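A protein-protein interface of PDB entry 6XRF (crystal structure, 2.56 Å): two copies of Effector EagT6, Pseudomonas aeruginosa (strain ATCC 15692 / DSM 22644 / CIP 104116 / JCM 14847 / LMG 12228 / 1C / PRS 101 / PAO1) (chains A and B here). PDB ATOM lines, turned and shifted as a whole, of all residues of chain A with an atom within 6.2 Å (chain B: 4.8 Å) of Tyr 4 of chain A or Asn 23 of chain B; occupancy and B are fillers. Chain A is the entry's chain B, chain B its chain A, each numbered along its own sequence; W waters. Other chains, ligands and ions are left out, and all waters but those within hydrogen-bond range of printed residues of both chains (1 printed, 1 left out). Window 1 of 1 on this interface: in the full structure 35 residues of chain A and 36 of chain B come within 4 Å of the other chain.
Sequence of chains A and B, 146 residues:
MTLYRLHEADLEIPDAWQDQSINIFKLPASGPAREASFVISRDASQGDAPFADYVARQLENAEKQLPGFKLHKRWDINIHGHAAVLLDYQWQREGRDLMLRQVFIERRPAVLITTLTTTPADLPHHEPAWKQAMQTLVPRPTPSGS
Tyr 4 of chain A touches His 7 of chain B.
CE1 of Tyr 4 of chain A touches CZ of Phe 25 of chain B, at 3.8 Å.
CD1 of Leu 6 of chain A touches OD1 of Asn 23 of chain B, at 3.9 Å.
Leu 6 of chain A touches Arg 42 of chain B (CD1 to NH2, 3.5 Å).
CE2 of Phe 38 of chain B touches CD1 of Leu 11 of chain A, at 3.9 Å.
CG2 of Ile 13 of chain A touches CD2 of Phe 25 of chain B, at 3.8 Å.
Ile 24 of chain B touches Asp 19 of chain A (O to OD1, 3.5 Å).
Ser 21 of chain A touches Ile 22 of chain B (CA to O, 3.5 Å).
Ser 21 of chain A touches Asn 23 of chain B (OG to CA, 3.3 Å).
CA of Ser 21 of chain B touches O of Ile 22 of chain A (3.6 Å).
The backbone carbonyl oxygen (O) of Ser 21 of chain B lies within hydrogen-bond range of the guanidinium group (NH1) of Arg 42 of chain B, 3.1 Å away.
NH1 of Arg 42 of chain B lies within hydrogen-bond range of O of Ile 40 of chain B.
The guanidinium group of Arg 5 of chain A lies within salt-bridge range of the side-chain carboxylate of Asp 10 of chain A.
The side-chain carboxylate (OD1) of Asp 19 of chain A lies within hydrogen-bond range of the side-chain hydroxyl (OG) of Ser 21 of chain A (2.7 Å).
The backbone carbonyl oxygen of Ser 21 of chain A sits at hydrogen-bond distance from the guanidinium group of Arg 42 of chain A.
The side-chain amide oxygen (OD1) of Asn 23 of chain A lies within hydrogen-bond range of the guanidinium group (NH2) of Arg 42 of chain A.
Water W1 bridges the guanidinium group of Arg 42 of chain B (3.4 Å) and the side-chain amide nitrogen of Asn 23 of chain A (3.5 Å).
The backbone NH (N) of His 7 of chain B sits at hydrogen-bond distance from the backbone carbonyl oxygen (O) of Arg 5 of chain A, at 3.0 Å.
The side-chain hydroxyl (OG) of Ser 21 of chain B sits at hydrogen-bond distance from the side-chain amide nitrogen (ND2) of Asn 23 of chain A, 3.2 Å away.
O of Ile 22 of chain B lies within hydrogen-bond range of N of Ile 22 of chain A (2.9 Å).
The side-chain amide nitrogen (ND2) of Asn 23 of chain B is in hydrogen-bond range of the side-chain hydroxyl (OH) of Tyr 4 of chain A (2.8 Å).
The backbone carbonyl oxygen of Ile 24 of chain B lies within hydrogen-bond range of the backbone NH of Gln 20 of chain A, at 2.7 Å.
The backbone NH of Ile 24 of chain B sits at hydrogen-bond distance from the side-chain hydroxyl of Ser 21 of chain A (3.3 Å).
The guanidinium group (NH2) of Arg 42 of chain B is in salt-bridge range of the side-chain carboxylate (OE1) of Glu 8 of chain A, at 3.3 Å.
Tyr 4 of chain A touches three residues of chain B.
Printed residues of chain B within 4 Å of Arg 5 of chain A: His 7.
Ala 9 of chain A touches none of the printed residues of chain B.
Printed residues of chain B within 4 Å of Ser 21 of chain A: Ile 22 (3.5 Å), Asn 23 (3.3 Å) and Ile 24 (3.3 Å).
Printed residues of chain A within 4 Å of His 7 of chain B: Leu 3, Tyr 4 and Arg 5.
Asn 23 of chain B touches just these residues of chain A: Tyr 4 (2.8 Å), Leu 6 (3.9 Å) and Ser 21 (3.3 Å).
The nearest printed residue of chain B that does not touch Tyr 4 of chain A is Ile 40 of chain B (5.3 Å).
The nearest residue of chain A that does not touch Asn 23 of chain B is Ile 22 of chain A (4.9 Å).
Ser 21 of chain A touches Ile 22 of chain B, and with the chains exchanged Ile 22 of chain A touches Ser 21 of chain B.
Ser 21 of chain A touches Asn 23 of chain B, and with the chains exchanged Asn 23 of chain A touches Ser 21 of chain B.
Ile 22 of chain A touches its own counterpart, Ile 22 of chain B.
Of the 18 pairs that touch across the chains among the printed residues, 5 have their exchanged pair printed and touching as well.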
ATOM      1  N   THR A   2      14.687 -26.828   4.033  1.00  0.00           N
ATOM      2  CA  THR A   2      14.292 -26.661   5.430  1.00  0.00           C
ATOM      3  C   THR A   2      13.496 -25.364   5.576  1.00  0.00           C
ATOM      4  O   THR A   2      14.033 -24.334   5.984  1.00  0.00           O
ATOM      5  CB  THR A   2      15.513 -26.646   6.363  1.00  0.00           C
ATOM      6  OG1 THR A   2      16.377 -27.746   6.042  1.00  0.00           O
ATOM      7  CG2 THR A   2      15.077 -26.762   7.818  1.00  0.00           C
ATOM      8  N   LEU A   3      12.211 -25.429   5.231  1.00  0.00           N
ATOM      9  CA  LEU A   3      11.338 -24.263   5.269  1.00  0.00           C
ATOM     10  C   LEU A   3      10.875 -24.004   6.697  1.00  0.00           C
ATOM     11  O   LEU A   3      10.441 -24.927   7.394  1.00  0.00           O
ATOM     12  CB  LEU A   3      10.137 -24.481   4.347  1.00  0.00           C
ATOM     13  CG  LEU A   3       9.170 -23.325   4.097  1.00  0.00           C
ATOM     14  CD1 LEU A   3       8.314 -23.614   2.861  1.00  0.00           C
ATOM     15  CD2 LEU A   3       8.274 -23.071   5.294  1.00  0.00           C
ATOM     16  N   TYR A   4      10.964 -22.749   7.131  1.00  0.00           N
ATOM     17  CA  TYR A   4      10.537 -22.344   8.465  1.00  0.00           C
ATOM     18  C   TYR A   4       9.238 -21.557   8.362  1.00  0.00           C
ATOM     19  O   TYR A   4       9.128 -20.631   7.552  1.00  0.00           O
ATOM     20  CB  TYR A   4      11.615 -21.504   9.155  1.00  0.00           C
ATOM     21  CG  TYR A   4      11.314 -21.201  10.608  1.00  0.00           C
ATOM     22  CD1 TYR A   4      10.695 -20.012  10.978  1.00  0.00           C
ATOM     23  CD2 TYR A   4      11.647 -22.103  11.613  1.00  0.00           C
ATOM     24  CE1 TYR A   4      10.416 -19.731  12.304  1.00  0.00           C
ATOM     25  CE2 TYR A   4      11.374 -21.829  12.941  1.00  0.00           C
ATOM     26  CZ  TYR A   4      10.757 -20.644  13.281  1.00  0.00           C
ATOM     27  OH  TYR A   4      10.482 -20.375  14.604  1.00  0.00           O
ATOM     28  N   ARG A   5       8.261 -21.930   9.187  1.00  0.00           N
ATOM     29  CA  ARG A   5       6.932 -21.328   9.175  1.00  0.00           C
ATOM     30  C   ARG A   5       6.762 -20.444  10.404  1.00  0.00           C
ATOM     31  O   ARG A   5       6.930 -20.911  11.536  1.00  0.00           O
ATOM     32  CB  ARG A   5       5.846 -22.405   9.152  1.00  0.00           C
ATOM     33  CG  ARG A   5       5.835 -23.259   7.903  1.00  0.00           C
ATOM     34  CD  ARG A   5       4.532 -23.085   7.129  1.00  0.00           C
ATOM     35  NE  ARG A   5       4.626 -23.616   5.772  1.00  0.00           N
ATOM     36  CZ  ARG A   5       4.129 -24.785   5.374  1.00  0.00           C
ATOM     37  NH1 ARG A   5       3.484 -25.574   6.225  1.00  0.00           N
ATOM     38  NH2 ARG A   5       4.277 -25.164   4.112  1.00  0.00           N
ATOM     39  N   LEU A   6       6.411 -19.180  10.183  1.00  0.00           N
ATOM     40  CA  LEU A   6       6.030 -18.275  11.254  1.00  0.00           C
ATOM     41  C   LEU A   6       4.683 -17.652  10.918  1.00  0.00           C
ATOM     42  O   LEU A   6       4.168 -17.790   9.804  1.00  0.00           O
ATOM     43  CB  LEU A   6       7.084 -17.188  11.490  1.00  0.00           C
ATOM     44  CG  LEU A   6       7.427 -16.237  10.349  1.00  0.00           C
ATOM     45  CD1 LEU A   6       7.666 -14.834  10.895  1.00  0.00           C
ATOM     46  CD2 LEU A   6       8.653 -16.722   9.600  1.00  0.00           C
ATOM     47  N   GLU A   8       3.710 -14.852  10.162  1.00  0.00           N
ATOM     48  CA  GLU A   8       3.647 -13.796   9.172  1.00  0.00           C
ATOM     49  C   GLU A   8       4.332 -14.130   7.856  1.00  0.00           C
ATOM     50  O   GLU A   8       4.218 -13.342   6.910  1.00  0.00           O
ATOM     51  CB  GLU A   8       4.273 -12.509   9.744  1.00  0.00           C
ATOM     52  CG  GLU A   8       3.535 -11.933  10.946  1.00  0.00           C
ATOM     53  CD  GLU A   8       4.125 -12.359  12.286  1.00  0.00           C
ATOM     54  OE1 GLU A   8       4.929 -13.317  12.327  1.00  0.00           O
ATOM     55  OE2 GLU A   8       3.782 -11.724  13.308  1.00  0.00           O
ATOM     56  N   ALA A   9       5.021 -15.264   7.755  1.00  0.00           N
ATOM     57  CA  ALA A   9       5.752 -15.540   6.528  1.00  0.00           C
ATOM     58  C   ALA A   9       6.311 -16.953   6.524  1.00  0.00           C
ATOM     59  O   ALA A   9       6.353 -17.638   7.548  1.00  0.00           O
ATOM     60  CB  ALA A   9       6.894 -14.532   6.339  1.00  0.00           C
ATOM     61  N   ASP A  10       6.741 -17.369   5.335  1.00  0.00           N
ATOM     62  CA  ASP A  10       7.526 -18.571   5.111  1.00  0.00           C
ATOM     63  C   ASP A  10       8.929 -18.158   4.688  1.00  0.00           C
ATOM     64  O   ASP A  10       9.112 -17.126   4.038  1.00  0.00           O
ATOM     65  CB  ASP A  10       6.903 -19.441   4.019  1.00  0.00           C
ATOM     66  CG  ASP A  10       5.401 -19.566   4.159  1.00  0.00           C
ATOM     67  OD1 ASP A  10       4.942 -20.427   4.940  1.00  0.00           O
ATOM     68  OD2 ASP A  10       4.683 -18.787   3.492  1.00  0.00           O
ATOM     69  N   LEU A  11       9.924 -18.961   5.049  1.00  0.00           N
ATOM     70  CA  LEU A  11      11.270 -18.723   4.545  1.00  0.00           C
ATOM     71  C   LEU A  11      12.099 -19.988   4.705  1.00  0.00           C
ATOM     72  O   LEU A  11      11.823 -20.832   5.561  1.00  0.00           O
ATOM     73  CB  LEU A  11      11.948 -17.543   5.253  1.00  0.00           C
ATOM     74  CG  LEU A  11      12.714 -17.773   6.556  1.00  0.00           C
ATOM     75  CD1 LEU A  11      13.575 -16.545   6.873  1.00  0.00           C
ATOM     76  CD2 LEU A  11      11.778 -18.071   7.704  1.00  0.00           C
ATOM     77  N   GLU A  12      13.124 -20.103   3.866  1.00  0.00           N
ATOM     78  CA  GLU A  12      14.058 -21.220   3.919  1.00  0.00           C
ATOM     79  C   GLU A  12      15.221 -20.855   4.836  1.00  0.00           C
ATOM     80  O   GLU A  12      15.882 -19.830   4.627  1.00  0.00           O
ATOM     81  CB  GLU A  12      14.568 -21.572   2.523  1.00  0.00           C
ATOM     82  CG  GLU A  12      13.638 -22.463   1.706  1.00  0.00           C
ATOM     83  CD  GLU A  12      12.535 -21.689   1.007  1.00  0.00           C
ATOM     84  OE1 GLU A  12      11.934 -20.798   1.643  1.00  0.00           O
ATOM     85  OE2 GLU A  12      12.274 -21.971  -0.185  1.00  0.00           O
ATOM     86  N   ILE A  13      15.470 -21.686   5.841  1.00  0.00           N
ATOM     87  CA  ILE A  13      16.572 -21.503   6.775  1.00  0.00           C
ATOM     88  C   ILE A  13      17.513 -22.691   6.617  1.00  0.00           C
ATOM     89  O   ILE A  13      17.057 -23.834   6.664  1.00  0.00           O
ATOM     90  CB  ILE A  13      16.096 -21.393   8.236  1.00  0.00           C
ATOM     91  CG1 ILE A  13      15.197 -20.164   8.420  1.00  0.00           C
ATOM     92  CG2 ILE A  13      17.286 -21.342   9.191  1.00  0.00           C
ATOM     93  CD1 ILE A  13      15.879 -18.843   8.133  1.00  0.00           C
ATOM     94  N   ASP A  19      18.078 -22.935  15.774  1.00  0.00           N
ATOM     95  CA  ASP A  19      16.824 -22.296  16.158  1.00  0.00           C
ATOM     96  C   ASP A  19      16.828 -22.014  17.657  1.00  0.00           C
ATOM     97  O   ASP A  19      17.020 -22.928  18.465  1.00  0.00           O
ATOM     98  CB  ASP A  19      15.646 -23.191  15.777  1.00  0.00           C
ATOM     99  CG  ASP A  19      14.307 -22.496  15.932  1.00  0.00           C
ATOM    100  OD1 ASP A  19      14.287 -21.337  16.391  1.00  0.00           O
ATOM    101  OD2 ASP A  19      13.275 -23.111  15.591  1.00  0.00           O
ATOM    102  N   GLN A  20      16.634 -20.744  18.028  1.00  0.00           N
ATOM    103  CA  GLN A  20      16.484 -20.347  19.423  1.00  0.00           C
ATOM    104  C   GLN A  20      15.231 -19.496  19.621  1.00  0.00           C
ATOM    105  O   GLN A  20      15.189 -18.641  20.510  1.00  0.00           O
ATOM    106  CB  GLN A  20      17.701 -19.568  19.922  1.00  0.00           C
ATOM    107  CG  GLN A  20      19.044 -20.244  19.754  1.00  0.00           C
ATOM    108  CD  GLN A  20      20.177 -19.408  20.341  1.00  0.00           C
ATOM    109  OE1 GLN A  20      20.070 -18.184  20.455  1.00  0.00           O
ATOM    110  NE2 GLN A  20      21.261 -20.071  20.728  1.00  0.00           N
ATOM    111  N   SER A  21      14.206 -19.714  18.802  1.00  0.00           N
ATOM    112  CA  SER A  21      13.057 -18.822  18.783  1.00  0.00           C
ATOM    113  C   SER A  21      12.276 -18.877  20.093  1.00  0.00           C
ATOM    114  O   SER A  21      12.216 -19.908  20.769  1.00  0.00           O
ATOM    115  CB  SER A  21      12.124 -19.180  17.623  1.00  0.00           C
ATOM    116  OG  SER A  21      12.814 -19.132  16.387  1.00  0.00           O
ATOM    117  N   ILE A  22      11.655 -17.745  20.431  1.00  0.00           N
ATOM    118  CA  ILE A  22      10.845 -17.591  21.636  1.00  0.00           C
ATOM    119  C   ILE A  22       9.571 -16.849  21.231  1.00  0.00           C
ATOM    120  O   ILE A  22       9.635 -15.673  20.849  1.00  0.00           O
ATOM    121  CB  ILE A  22      11.577 -16.822  22.743  1.00  0.00           C
ATOM    122  CG1 ILE A  22      12.981 -17.384  22.981  1.00  0.00           C
ATOM    123  CG2 ILE A  22      10.757 -16.839  24.033  1.00  0.00           C
ATOM    124  CD1 ILE A  22      13.018 -18.767  23.592  1.00  0.00           C
ATOM    125  N   ASN A  23       8.419 -17.517  21.325  1.00  0.00           N
ATOM    126  CA  ASN A  23       7.143 -16.825  21.163  1.00  0.00           C
ATOM    127  C   ASN A  23       6.735 -16.192  22.485  1.00  0.00           C
ATOM    128  O   ASN A  23       6.853 -16.811  23.547  1.00  0.00           O
ATOM    129  CB  ASN A  23       6.056 -17.786  20.690  1.00  0.00           C
ATOM    130  CG  ASN A  23       6.247 -18.213  19.250  1.00  0.00           C
ATOM    131  OD1 ASN A  23       6.752 -19.305  18.986  1.00  0.00           O
ATOM    132  ND2 ASN A  23       5.846 -17.353  18.307  1.00  0.00           N
ATOM    133  N   ARG A  42      11.795 -23.576  23.124  1.00  0.00           N
ATOM    134  CA  ARG A  42      12.193 -24.900  22.683  1.00  0.00           C
ATOM    135  C   ARG A  42      13.416 -25.366  23.459  1.00  0.00           C
ATOM    136  O   ARG A  42      14.175 -24.565  24.013  1.00  0.00           O
ATOM    137  CB  ARG A  42      12.491 -24.925  21.180  1.00  0.00           C
ATOM    138  CG  ARG A  42      11.285 -24.646  20.295  1.00  0.00           C
ATOM    139  CD  ARG A  42      11.077 -23.154  20.062  1.00  0.00           C
ATOM    140  NE  ARG A  42       9.982 -22.896  19.127  1.00  0.00           N
ATOM    141  CZ  ARG A  42       9.166 -21.844  19.192  1.00  0.00           C
ATOM    142  NH1 ARG A  42       9.304 -20.942  20.159  1.00  0.00           N
ATOM    143  NH2 ARG A  42       8.197 -21.699  18.298  1.00  0.00           N
ATOM    144  N   HIS B   7       6.375 -22.556  13.990  1.00  0.00           N
ATOM    145  CA  HIS B   7       7.033 -23.597  13.218  1.00  0.00           C
ATOM    146  C   HIS B   7       6.561 -24.982  13.627  1.00  0.00           C
ATOM    147  O   HIS B   7       6.529 -25.884  12.791  1.00  0.00           O
ATOM    148  CB  HIS B   7       8.550 -23.492  13.377  1.00  0.00           C
ATOM    149  CG  HIS B   7       9.322 -24.365  12.439  1.00  0.00           C
ATOM    150  ND1 HIS B   7       9.139 -24.338  11.073  1.00  0.00           N
ATOM    151  CD2 HIS B   7      10.297 -25.278  12.668  1.00  0.00           C
ATOM    152  CE1 HIS B   7       9.967 -25.195  10.501  1.00  0.00           C
ATOM    153  NE2 HIS B   7      10.669 -25.789  11.448  1.00  0.00           N
ATOM    154  N   SER B  21       6.713 -11.846  19.867  1.00  0.00           N
ATOM    155  CA  SER B  21       7.476 -13.041  19.538  1.00  0.00           C
ATOM    156  C   SER B  21       8.722 -12.689  18.736  1.00  0.00           C
ATOM    157  O   SER B  21       8.750 -11.714  17.983  1.00  0.00           O
ATOM    158  CB  SER B  21       6.608 -14.027  18.757  1.00  0.00           C
ATOM    159  OG  SER B  21       5.458 -14.401  19.506  1.00  0.00           O
ATOM    160  N   ILE B  22       9.766 -13.499  18.918  1.00  0.00           N
ATOM    161  CA  ILE B  22      11.062 -13.282  18.288  1.00  0.00           C
ATOM    162  C   ILE B  22      11.576 -14.624  17.788  1.00  0.00           C
ATOM    163  O   ILE B  22      11.816 -15.533  18.589  1.00  0.00           O
ATOM    164  CB  ILE B  22      12.099 -12.679  19.253  1.00  0.00           C
ATOM    165  CG1 ILE B  22      11.534 -11.484  20.012  1.00  0.00           C
ATOM    166  CG2 ILE B  22      13.357 -12.272  18.495  1.00  0.00           C
ATOM    167  CD1 ILE B  22      11.469 -11.718  21.513  1.00  0.00           C
ATOM    168  N   ASN B  23      11.761 -14.750  16.478  1.00  0.00           N
ATOM    169  CA  ASN B  23      12.484 -15.883  15.918  1.00  0.00           C
ATOM    170  C   ASN B  23      13.969 -15.556  15.920  1.00  0.00           C
ATOM    171  O   ASN B  23      14.377 -14.439  15.588  1.00  0.00           O
ATOM    172  CB  ASN B  23      12.001 -16.190  14.505  1.00  0.00           C
ATOM    173  CG  ASN B  23      10.511 -16.399  14.445  1.00  0.00           C
ATOM    174  OD1 ASN B  23       9.763 -15.484  14.114  1.00  0.00           O
ATOM    175  ND2 ASN B  23      10.064 -17.599  14.791  1.00  0.00           N
ATOM    176  N   ILE B  24      14.774 -16.533  16.324  1.00  0.00           N
ATOM    177  CA  ILE B  24      16.208 -16.353  16.517  1.00  0.00           C
ATOM    178  C   ILE B  24      16.926 -17.540  15.899  1.00  0.00           C
ATOM    179  O   ILE B  24      16.621 -18.693  16.223  1.00  0.00           O
ATOM    180  CB  ILE B  24      16.571 -16.228  18.010  1.00  0.00           C
ATOM    181  CG1 ILE B  24      15.980 -14.950  18.607  1.00  0.00           C
ATOM    182  CG2 ILE B  24      18.079 -16.244  18.197  1.00  0.00           C
ATOM    183  CD1 ILE B  24      15.942 -14.947  20.128  1.00  0.00           C
ATOM    184  N   PHE B  25      17.873 -17.262  15.013  1.00  0.00           N
ATOM    185  CA  PHE B  25      18.723 -18.287  14.423  1.00  0.00           C
ATOM    186  C   PHE B  25      20.161 -17.830  14.585  1.00  0.00           C
ATOM    187  O   PHE B  25      20.492 -16.687  14.255  1.00  0.00           O
ATOM    188  CB  PHE B  25      18.380 -18.518  12.949  1.00  0.00           C
ATOM    189  CG  PHE B  25      16.922 -18.777  12.712  1.00  0.00           C
ATOM    190  CD1 PHE B  25      16.030 -17.721  12.604  1.00  0.00           C
ATOM    191  CD2 PHE B  25      16.436 -20.070  12.615  1.00  0.00           C
ATOM    192  CE1 PHE B  25      14.683 -17.949  12.398  1.00  0.00           C
ATOM    193  CE2 PHE B  25      15.084 -20.306  12.405  1.00  0.00           C
ATOM    194  CZ  PHE B  25      14.209 -19.243  12.299  1.00  0.00           C
ATOM    195  N   PHE B  38      20.752 -14.192  13.056  1.00  0.00           N
ATOM    196  CA  PHE B  38      19.659 -13.738  12.207  1.00  0.00           C
ATOM    197  C   PHE B  38      18.388 -13.762  13.039  1.00  0.00           C
ATOM    198  O   PHE B  38      18.023 -14.811  13.581  1.00  0.00           O
ATOM    199  CB  PHE B  38      19.514 -14.623  10.969  1.00  0.00           C
ATOM    200  CG  PHE B  38      18.352 -14.253  10.102  1.00  0.00           C
ATOM    201  CD1 PHE B  38      18.316 -13.029   9.459  1.00  0.00           C
ATOM    202  CD2 PHE B  38      17.294 -15.126   9.929  1.00  0.00           C
ATOM    203  CE1 PHE B  38      17.248 -12.683   8.665  1.00  0.00           C
ATOM    204  CE2 PHE B  38      16.221 -14.783   9.136  1.00  0.00           C
ATOM    205  CZ  PHE B  38      16.199 -13.561   8.505  1.00  0.00           C
ATOM    206  N   VAL B  39      17.717 -12.618  13.143  1.00  0.00           N
ATOM    207  CA  VAL B  39      16.608 -12.447  14.072  1.00  0.00           C
ATOM    208  C   VAL B  39      15.412 -11.865  13.335  1.00  0.00           C
ATOM    209  O   VAL B  39      15.556 -10.900  12.577  1.00  0.00           O
ATOM    210  CB  VAL B  39      16.993 -11.541  15.256  1.00  0.00           C
ATOM    211  CG1 VAL B  39      15.768 -11.194  16.084  1.00  0.00           C
ATOM    212  CG2 VAL B  39      18.057 -12.215  16.101  1.00  0.00           C
ATOM    213  N   ILE B  40      14.236 -12.435  13.582  1.00  0.00           N
ATOM    214  CA  ILE B  40      12.974 -11.931  13.058  1.00  0.00           C
ATOM    215  C   ILE B  40      12.186 -11.376  14.236  1.00  0.00           C
ATOM    216  O   ILE B  40      11.880 -12.106  15.187  1.00  0.00           O
ATOM    217  CB  ILE B  40      12.184 -13.026  12.330  1.00  0.00           C
ATOM    218  CG1 ILE B  40      13.077 -13.732  11.309  1.00  0.00           C
ATOM    219  CG2 ILE B  40      10.976 -12.416  11.637  1.00  0.00           C
ATOM    220  CD1 ILE B  40      12.463 -14.986  10.714  1.00  0.00           C
ATOM    221  N   ARG B  42       9.022  -8.249  15.444  1.00  0.00           N
ATOM    222  CA  ARG B  42       7.845  -7.532  14.981  1.00  0.00           C
ATOM    223  C   ARG B  42       7.751  -6.180  15.676  1.00  0.00           C
ATOM    224  O   ARG B  42       8.200  -6.015  16.816  1.00  0.00           O
ATOM    225  CB  ARG B  42       6.554  -8.321  15.229  1.00  0.00           C
ATOM    226  CG  ARG B  42       6.531  -9.701  14.597  1.00  0.00           C
ATOM    227  CD  ARG B  42       6.785 -10.781  15.638  1.00  0.00           C
ATOM    228  NE  ARG B  42       6.653 -12.126  15.087  1.00  0.00           N
ATOM    229  CZ  ARG B  42       7.673 -12.936  14.818  1.00  0.00           C
ATOM    230  NH1 ARG B  42       8.923 -12.551  15.047  1.00  0.00           N
ATOM    231  NH2 ARG B  42       7.438 -14.144  14.322  1.00  0.00           N
HETATM  232  O   HOH W   1       5.241 -16.685  14.931  1.00  0.00           O
